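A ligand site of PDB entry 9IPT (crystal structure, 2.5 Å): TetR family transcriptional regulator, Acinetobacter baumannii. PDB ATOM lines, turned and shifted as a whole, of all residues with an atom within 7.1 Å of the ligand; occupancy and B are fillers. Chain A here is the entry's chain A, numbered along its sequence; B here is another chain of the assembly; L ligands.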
ATOM      1  N   MET A  64      10.654 -26.090  27.340  1.00  0.00           N
ATOM      2  CA  MET A  64      10.956 -24.673  27.182  1.00  0.00           C
ATOM      3  C   MET A  64      11.392 -24.060  28.511  1.00  0.00           C
ATOM      4  O   MET A  64      12.248 -23.167  28.544  1.00  0.00           O
ATOM      5  CB  MET A  64       9.742 -23.929  26.619  1.00  0.00           C
ATOM      6  CG  MET A  64       9.250 -24.496  25.307  1.00  0.00           C
ATOM      7  SD  MET A  64      10.332 -24.061  23.923  1.00  0.00           S
ATOM      8  CE  MET A  64      11.107 -25.632  23.597  1.00  0.00           C
ATOM      9  N   LEU A  67      14.921 -24.926  28.564  1.00  0.00           N
ATOM     10  CA  LEU A  67      15.616 -23.916  27.773  1.00  0.00           C
ATOM     11  C   LEU A  67      15.801 -22.628  28.559  1.00  0.00           C
ATOM     12  O   LEU A  67      16.891 -22.034  28.554  1.00  0.00           O
ATOM     13  CB  LEU A  67      14.825 -23.654  26.487  1.00  0.00           C
ATOM     14  CG  LEU A  67      15.279 -22.447  25.641  1.00  0.00           C
ATOM     15  CD1 LEU A  67      16.447 -22.805  24.744  1.00  0.00           C
ATOM     16  CD2 LEU A  67      14.120 -21.907  24.831  1.00  0.00           C
ATOM     17  N   ASP A  68      14.749 -22.180  29.235  1.00  0.00           N
ATOM     18  CA  ASP A  68      14.842 -20.969  30.064  1.00  0.00           C
ATOM     19  C   ASP A  68      15.869 -21.149  31.167  1.00  0.00           C
ATOM     20  O   ASP A  68      16.671 -20.254  31.442  1.00  0.00           O
ATOM     21  CB  ASP A  68      13.446 -20.624  30.610  1.00  0.00           C
ATOM     22  CG  ASP A  68      13.468 -19.517  31.671  1.00  0.00           C
ATOM     23  OD1 ASP A  68      14.211 -19.592  32.673  1.00  0.00           O
ATOM     24  OD2 ASP A  68      12.645 -18.587  31.538  1.00  0.00           O
ATOM     25  N   GLU A  71      19.290 -21.002  30.036  1.00  0.00           N
ATOM     26  CA  GLU A  71      19.467 -19.654  29.499  1.00  0.00           C
ATOM     27  C   GLU A  71      19.828 -18.630  30.564  1.00  0.00           C
ATOM     28  O   GLU A  71      20.358 -17.558  30.221  1.00  0.00           O
ATOM     29  CB  GLU A  71      18.185 -19.209  28.786  1.00  0.00           C
ATOM     30  CG  GLU A  71      18.265 -19.298  27.270  1.00  0.00           C
ATOM     31  CD  GLU A  71      17.030 -18.743  26.579  1.00  0.00           C
ATOM     32  OE1 GLU A  71      16.036 -18.465  27.272  1.00  0.00           O
ATOM     33  OE2 GLU A  71      17.065 -18.585  25.341  1.00  0.00           O
ATOM     34  N   ILE A  85      20.923 -13.316  23.199  1.00  0.00           N
ATOM     35  CA  ILE A  85      20.641 -14.739  23.347  1.00  0.00           C
ATOM     36  C   ILE A  85      19.183 -14.959  23.707  1.00  0.00           C
ATOM     37  O   ILE A  85      18.538 -15.901  23.225  1.00  0.00           O
ATOM     38  CB  ILE A  85      21.590 -15.358  24.389  1.00  0.00           C
ATOM     39  CG1 ILE A  85      22.980 -15.591  23.781  1.00  0.00           C
ATOM     40  CG2 ILE A  85      21.033 -16.663  24.929  1.00  0.00           C
ATOM     41  CD1 ILE A  85      24.120 -15.220  24.707  1.00  0.00           C
ATOM     42  N   LEU A  86      18.629 -14.086  24.552  1.00  0.00           N
ATOM     43  CA  LEU A  86      17.244 -14.246  24.997  1.00  0.00           C
ATOM     44  C   LEU A  86      16.266 -14.163  23.835  1.00  0.00           C
ATOM     45  O   LEU A  86      15.195 -14.783  23.883  1.00  0.00           O
ATOM     46  CB  LEU A  86      16.915 -13.180  26.051  1.00  0.00           C
ATOM     47  CG  LEU A  86      17.181 -13.506  27.524  1.00  0.00           C
ATOM     48  CD1 LEU A  86      15.956 -13.201  28.361  1.00  0.00           C
ATOM     49  CD2 LEU A  86      17.625 -14.954  27.712  1.00  0.00           C
ATOM     50  N   LEU A  87      16.603 -13.414  22.790  1.00  0.00           N
ATOM     51  CA  LEU A  87      15.751 -13.308  21.616  1.00  0.00           C
ATOM     52  C   LEU A  87      15.896 -14.485  20.660  1.00  0.00           C
ATOM     53  O   LEU A  87      15.195 -14.536  19.647  1.00  0.00           O
ATOM     54  CB  LEU A  87      16.050 -12.008  20.858  1.00  0.00           C
ATOM     55  CG  LEU A  87      15.593 -10.703  21.517  1.00  0.00           C
ATOM     56  CD1 LEU A  87      16.433  -9.544  21.001  1.00  0.00           C
ATOM     57  CD2 LEU A  87      14.125 -10.450  21.257  1.00  0.00           C
ATOM     58  N   GLY A  88      16.785 -15.431  20.955  1.00  0.00           N
ATOM     59  CA  GLY A  88      17.064 -16.494  20.016  1.00  0.00           C
ATOM     60  C   GLY A  88      17.792 -16.040  18.778  1.00  0.00           C
ATOM     61  O   GLY A  88      17.716 -16.710  17.744  1.00  0.00           O
ATOM     62  N   ALA A  89      18.500 -14.916  18.846  1.00  0.00           N
ATOM     63  CA  ALA A  89      19.231 -14.374  17.712  1.00  0.00           C
ATOM     64  C   ALA A  89      20.678 -14.837  17.660  1.00  0.00           C
ATOM     65  O   ALA A  89      21.338 -14.657  16.625  1.00  0.00           O
ATOM     66  CB  ALA A  89      19.192 -12.838  17.732  1.00  0.00           C
ATOM     67  N   LEU A  95      21.401 -25.218  21.754  1.00  0.00           N
ATOM     68  CA  LEU A  95      20.035 -24.746  21.887  1.00  0.00           C
ATOM     69  C   LEU A  95      19.205 -24.863  20.610  1.00  0.00           C
ATOM     70  O   LEU A  95      18.006 -24.558  20.642  1.00  0.00           O
ATOM     71  CB  LEU A  95      20.013 -23.282  22.358  1.00  0.00           C
ATOM     72  CG  LEU A  95      20.371 -23.041  23.821  1.00  0.00           C
ATOM     73  CD1 LEU A  95      19.985 -21.619  24.246  1.00  0.00           C
ATOM     74  CD2 LEU A  95      19.725 -24.085  24.720  1.00  0.00           C
ATOM     75  N   TYR A  98      15.988 -27.123  21.123  1.00  0.00           N
ATOM     76  CA  TYR A  98      14.862 -26.455  21.793  1.00  0.00           C
ATOM     77  C   TYR A  98      14.220 -25.410  20.902  1.00  0.00           C
ATOM     78  O   TYR A  98      13.001 -25.221  20.948  1.00  0.00           O
ATOM     79  CB  TYR A  98      15.321 -25.820  23.101  1.00  0.00           C
ATOM     80  CG  TYR A  98      15.959 -26.771  24.090  1.00  0.00           C
ATOM     81  CD1 TYR A  98      17.249 -27.249  23.893  1.00  0.00           C
ATOM     82  CD2 TYR A  98      15.273 -27.183  25.230  1.00  0.00           C
ATOM     83  CE1 TYR A  98      17.831 -28.120  24.790  1.00  0.00           C
ATOM     84  CE2 TYR A  98      15.854 -28.055  26.128  1.00  0.00           C
ATOM     85  CZ  TYR A  98      17.138 -28.522  25.912  1.00  0.00           C
ATOM     86  OH  TYR A  98      17.718 -29.379  26.808  1.00  0.00           O
ATOM     87  N   LEU A  99      15.012 -24.725  20.076  1.00  0.00           N
ATOM     88  CA  LEU A  99      14.450 -23.738  19.164  1.00  0.00           C
ATOM     89  C   LEU A  99      13.708 -24.393  18.010  1.00  0.00           C
ATOM     90  O   LEU A  99      12.712 -23.853  17.522  1.00  0.00           O
ATOM     91  CB  LEU A  99      15.555 -22.820  18.633  1.00  0.00           C
ATOM     92  CG  LEU A  99      15.871 -21.531  19.398  1.00  0.00           C
ATOM     93  CD1 LEU A  99      15.805 -21.736  20.912  1.00  0.00           C
ATOM     94  CD2 LEU A  99      17.240 -21.011  19.003  1.00  0.00           C
ATOM     95  N   TRP A 102      10.341 -25.313  19.376  1.00  0.00           N
ATOM     96  CA  TRP A 102       9.498 -24.113  19.463  1.00  0.00           C
ATOM     97  C   TRP A 102       8.895 -23.778  18.110  1.00  0.00           C
ATOM     98  O   TRP A 102       7.696 -23.488  17.999  1.00  0.00           O
ATOM     99  CB  TRP A 102      10.321 -22.937  19.995  1.00  0.00           C
ATOM    100  CG  TRP A 102       9.494 -21.830  20.585  1.00  0.00           C
ATOM    101  CD1 TRP A 102       8.292 -21.371  20.122  1.00  0.00           C
ATOM    102  CD2 TRP A 102       9.812 -21.036  21.741  1.00  0.00           C
ATOM    103  NE1 TRP A 102       7.841 -20.340  20.917  1.00  0.00           N
ATOM    104  CE2 TRP A 102       8.752 -20.119  21.917  1.00  0.00           C
ATOM    105  CE3 TRP A 102      10.883 -21.011  22.635  1.00  0.00           C
ATOM    106  CZ2 TRP A 102       8.732 -19.194  22.951  1.00  0.00           C
ATOM    107  CZ3 TRP A 102      10.852 -20.095  23.673  1.00  0.00           C
ATOM    108  CH2 TRP A 102       9.796 -19.195  23.828  1.00  0.00           C
ATOM    109  N   ASN A 103       9.717 -23.818  17.051  1.00  0.00           N
ATOM    110  CA  ASN A 103       9.204 -23.584  15.713  1.00  0.00           C
ATOM    111  C   ASN A 103       8.244 -24.678  15.273  1.00  0.00           C
ATOM    112  O   ASN A 103       7.288 -24.408  14.542  1.00  0.00           O
ATOM    113  CB  ASN A 103      10.365 -23.459  14.726  1.00  0.00           C
ATOM    114  CG  ASN A 103      11.208 -22.224  14.969  1.00  0.00           C
ATOM    115  OD1 ASN A 103      10.746 -21.243  15.546  1.00  0.00           O
ATOM    116  ND2 ASN A 103      12.453 -22.264  14.518  1.00  0.00           N
ATOM    117  N   GLU A 106       4.905 -24.006  16.675  1.00  0.00           N
ATOM    118  CA  GLU A 106       4.255 -22.854  16.062  1.00  0.00           C
ATOM    119  C   GLU A 106       3.267 -23.270  14.991  1.00  0.00           C
ATOM    120  O   GLU A 106       2.253 -22.589  14.771  1.00  0.00           O
ATOM    121  CB  GLU A 106       5.301 -21.909  15.480  1.00  0.00           C
ATOM    122  CG  GLU A 106       5.078 -20.447  15.833  1.00  0.00           C
ATOM    123  CD  GLU A 106       5.719 -19.488  14.853  1.00  0.00           C
ATOM    124  OE1 GLU A 106       6.896 -19.710  14.497  1.00  0.00           O
ATOM    125  OE2 GLU A 106       5.051 -18.516  14.443  1.00  0.00           O
ATOM    126  N   TYR A 119       1.966 -23.090  23.959  1.00  0.00           N
ATOM    127  CA  TYR A 119       2.712 -22.134  23.147  1.00  0.00           C
ATOM    128  C   TYR A 119       2.523 -20.708  23.662  1.00  0.00           C
ATOM    129  O   TYR A 119       3.484 -19.944  23.790  1.00  0.00           O
ATOM    130  CB  TYR A 119       2.294 -22.247  21.682  1.00  0.00           C
ATOM    131  CG  TYR A 119       3.023 -21.293  20.778  1.00  0.00           C
ATOM    132  CD1 TYR A 119       4.305 -21.575  20.316  1.00  0.00           C
ATOM    133  CD2 TYR A 119       2.439 -20.092  20.376  1.00  0.00           C
ATOM    134  CE1 TYR A 119       4.977 -20.705  19.485  1.00  0.00           C
ATOM    135  CE2 TYR A 119       3.109 -19.213  19.556  1.00  0.00           C
ATOM    136  CZ  TYR A 119       4.374 -19.517  19.107  1.00  0.00           C
ATOM    137  OH  TYR A 119       5.034 -18.640  18.279  1.00  0.00           O
ATOM    138  N   MET A 123       5.282 -18.265  25.312  1.00  0.00           N
ATOM    139  CA  MET A 123       5.459 -16.938  24.737  1.00  0.00           C
ATOM    140  C   MET A 123       5.367 -15.853  25.795  1.00  0.00           C
ATOM    141  O   MET A 123       6.103 -14.866  25.748  1.00  0.00           O
ATOM    142  CB  MET A 123       4.436 -16.694  23.622  1.00  0.00           C
ATOM    143  CG  MET A 123       5.033 -16.094  22.371  1.00  0.00           C
ATOM    144  SD  MET A 123       6.269 -17.153  21.602  1.00  0.00           S
ATOM    145  CE  MET A 123       6.414 -16.396  19.987  1.00  0.00           C
ATOM    146  N   TRP A 126       8.512 -15.938  27.708  1.00  0.00           N
ATOM    147  CA  TRP A 126       9.561 -15.332  26.893  1.00  0.00           C
ATOM    148  C   TRP A 126       9.510 -13.820  26.957  1.00  0.00           C
ATOM    149  O   TRP A 126      10.548 -13.148  26.944  1.00  0.00           O
ATOM    150  CB  TRP A 126       9.442 -15.813  25.447  1.00  0.00           C
ATOM    151  CG  TRP A 126      10.574 -15.374  24.552  1.00  0.00           C
ATOM    152  CD1 TRP A 126      11.870 -15.180  24.909  1.00  0.00           C
ATOM    153  CD2 TRP A 126      10.495 -15.083  23.160  1.00  0.00           C
ATOM    154  NE1 TRP A 126      12.607 -14.781  23.825  1.00  0.00           N
ATOM    155  CE2 TRP A 126      11.789 -14.715  22.735  1.00  0.00           C
ATOM    156  CE3 TRP A 126       9.462 -15.095  22.218  1.00  0.00           C
ATOM    157  CZ2 TRP A 126      12.071 -14.364  21.410  1.00  0.00           C
ATOM    158  CZ3 TRP A 126       9.743 -14.749  20.907  1.00  0.00           C
ATOM    159  CH2 TRP A 126      11.035 -14.383  20.518  1.00  0.00           C
ATOM    160  N   ILE A 157      10.189  -8.741  20.390  1.00  0.00           N
ATOM    161  CA  ILE A 157       9.677 -10.047  20.010  1.00  0.00           C
ATOM    162  C   ILE A 157       9.040  -9.981  18.626  1.00  0.00           C
ATOM    163  O   ILE A 157       9.235 -10.886  17.793  1.00  0.00           O
ATOM    164  CB  ILE A 157       8.685 -10.564  21.066  1.00  0.00           C
ATOM    165  CG1 ILE A 157       9.431 -11.220  22.227  1.00  0.00           C
ATOM    166  CG2 ILE A 157       7.691 -11.537  20.460  1.00  0.00           C
ATOM    167  CD1 ILE A 157       8.672 -11.214  23.524  1.00  0.00           C
ATOM    168  N   VAL A 160      11.971  -9.929  15.876  1.00  0.00           N
ATOM    169  CA  VAL A 160      12.687 -11.178  15.631  1.00  0.00           C
ATOM    170  C   VAL A 160      11.751 -12.239  15.051  1.00  0.00           C
ATOM    171  O   VAL A 160      12.178 -13.054  14.227  1.00  0.00           O
ATOM    172  CB  VAL A 160      13.382 -11.669  16.924  1.00  0.00           C
ATOM    173  CG1 VAL A 160      14.267 -10.579  17.499  1.00  0.00           C
ATOM    174  CG2 VAL A 160      12.359 -12.122  17.951  1.00  0.00           C
ATOM    175  N   CYS A 161      10.480 -12.234  15.442  1.00  0.00           N
ATOM    176  CA  CYS A 161       9.524 -13.138  14.826  1.00  0.00           C
ATOM    177  C   CYS A 161       9.171 -12.684  13.417  1.00  0.00           C
ATOM    178  O   CYS A 161       8.926 -13.519  12.536  1.00  0.00           O
ATOM    179  CB  CYS A 161       8.256 -13.226  15.682  1.00  0.00           C
ATOM    180  SG  CYS A 161       8.282 -14.527  16.940  1.00  0.00           S
ATOM    181  N   GLU A 164      12.113 -13.425  10.894  1.00  0.00           N
ATOM    182  CA  GLU A 164      12.181 -14.850  10.591  1.00  0.00           C
ATOM    183  C   GLU A 164      11.162 -15.208   9.505  1.00  0.00           C
ATOM    184  O   GLU A 164      11.442 -16.035   8.635  1.00  0.00           O
ATOM    185  CB  GLU A 164      11.923 -15.686  11.838  1.00  0.00           C
ATOM    186  CG  GLU A 164      13.153 -16.404  12.374  1.00  0.00           C
ATOM    187  CD  GLU A 164      13.289 -16.302  13.876  1.00  0.00           C
ATOM    188  OE1 GLU A 164      12.245 -16.199  14.561  1.00  0.00           O
ATOM    189  OE2 GLU A 164      14.431 -16.323  14.374  1.00  0.00           O
ATOM    190  N   LYS A 168      11.527 -16.758   5.325  1.00  0.00           N
ATOM    191  CA  LYS A 168      10.921 -17.961   4.756  1.00  0.00           C
ATOM    192  C   LYS A 168      10.441 -17.744   3.328  1.00  0.00           C
ATOM    193  O   LYS A 168      10.318 -18.722   2.582  1.00  0.00           O
ATOM    194  CB  LYS A 168       9.751 -18.408   5.632  1.00  0.00           C
ATOM    195  CG  LYS A 168      10.165 -19.128   6.905  1.00  0.00           C
ATOM    196  CD  LYS A 168       8.947 -19.478   7.750  1.00  0.00           C
ATOM    197  CE  LYS A 168       9.341 -19.816   9.175  1.00  0.00           C
ATOM    198  NZ  LYS A 168      10.590 -20.627   9.233  1.00  0.00           N
ATOM    199  N   ILE B 166       2.001 -11.609  15.947  1.00  0.00           N
ATOM    200  CA  ILE B 166       1.862 -11.798  17.399  1.00  0.00           C
ATOM    201  C   ILE B 166       0.426 -11.564  17.824  1.00  0.00           C
ATOM    202  O   ILE B 166      -0.066 -12.204  18.772  1.00  0.00           O
ATOM    203  CB  ILE B 166       2.840 -10.877  18.152  1.00  0.00           C
ATOM    204  CG1 ILE B 166       4.276 -11.131  17.688  1.00  0.00           C
ATOM    205  CG2 ILE B 166       2.736 -11.090  19.647  1.00  0.00           C
ATOM    206  CD1 ILE B 166       4.779 -12.525  17.990  1.00  0.00           C
HETATM  207  N1  LIG L   1      14.618 -18.125  24.295  1.00  0.00           N
HETATM  208  C1  LIG L   1      14.746 -18.138  22.855  1.00  0.00           C
HETATM  209  C2  LIG L   1      13.348 -18.054  22.294  1.00  0.00           C
HETATM  210  C3  LIG L   1      13.316 -18.063  20.785  1.00  0.00           C
HETATM  211  C4  LIG L   1      11.898 -18.302  20.339  1.00  0.00           C
HETATM  212  N2  LIG L   1      11.754 -17.968  18.956  1.00  0.00           N
HETATM  213  C5  LIG L   1      10.778 -18.643  18.155  1.00  0.00           C
HETATM  214  C6  LIG L   1       9.416 -18.005  18.285  1.00  0.00           C
HETATM  215  C7  LIG L   1       8.669 -18.066  16.971  1.00  0.00           C
HETATM  216  N3  LIG L   1       9.604 -18.054  15.874  1.00  0.00           N
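N1 of the ligand is in salt-bridge range of OE2 of Glu 71 (2.7 Å). A nitrogen (N3) of the ligand is in hydrogen-bond range of the side-chain amide oxygen of Asn 103 (3.4 Å). A nitrogen (N1) of the ligand is in hydrogen-bond range of the backbone carbonyl oxygen (O) of Leu 86 (3.4 Å). The side-chain carboxylate of Glu 106 is in salt-bridge range of a nitrogen (N3) of the ligand. The side-chain carboxylate (OE1) of Glu 164 lies within salt-bridge range of a nitrogen (N3) of the ligand, at 3.5 Å.
The side-chain amide nitrogen of Asn 103 sits close to the backbone carbonyl oxygen of Leu 99 (3.4 Å). NE1 of Trp 126 sits at hydrogen-bond distance from O of Leu 86 (2.6 Å). NE1 of Trp 102 sits close to SD of Met 123, at 3.6 Å.
Merely in contact with the ligand: Leu 67, Gly 88, Trp 102, Tyr 119, Met 123, Trp 126 and Cys 161. Within 4 Å of the ligand: Leu 67, Glu 71, Leu 86, Gly 88, Trp 102, Asn 103, Glu 106, Tyr 119, Met 123, Trp 126, Cys 161 and Glu 164. The nearest printed residue that does not touch the ligand is Leu 87 (4.2 Å).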
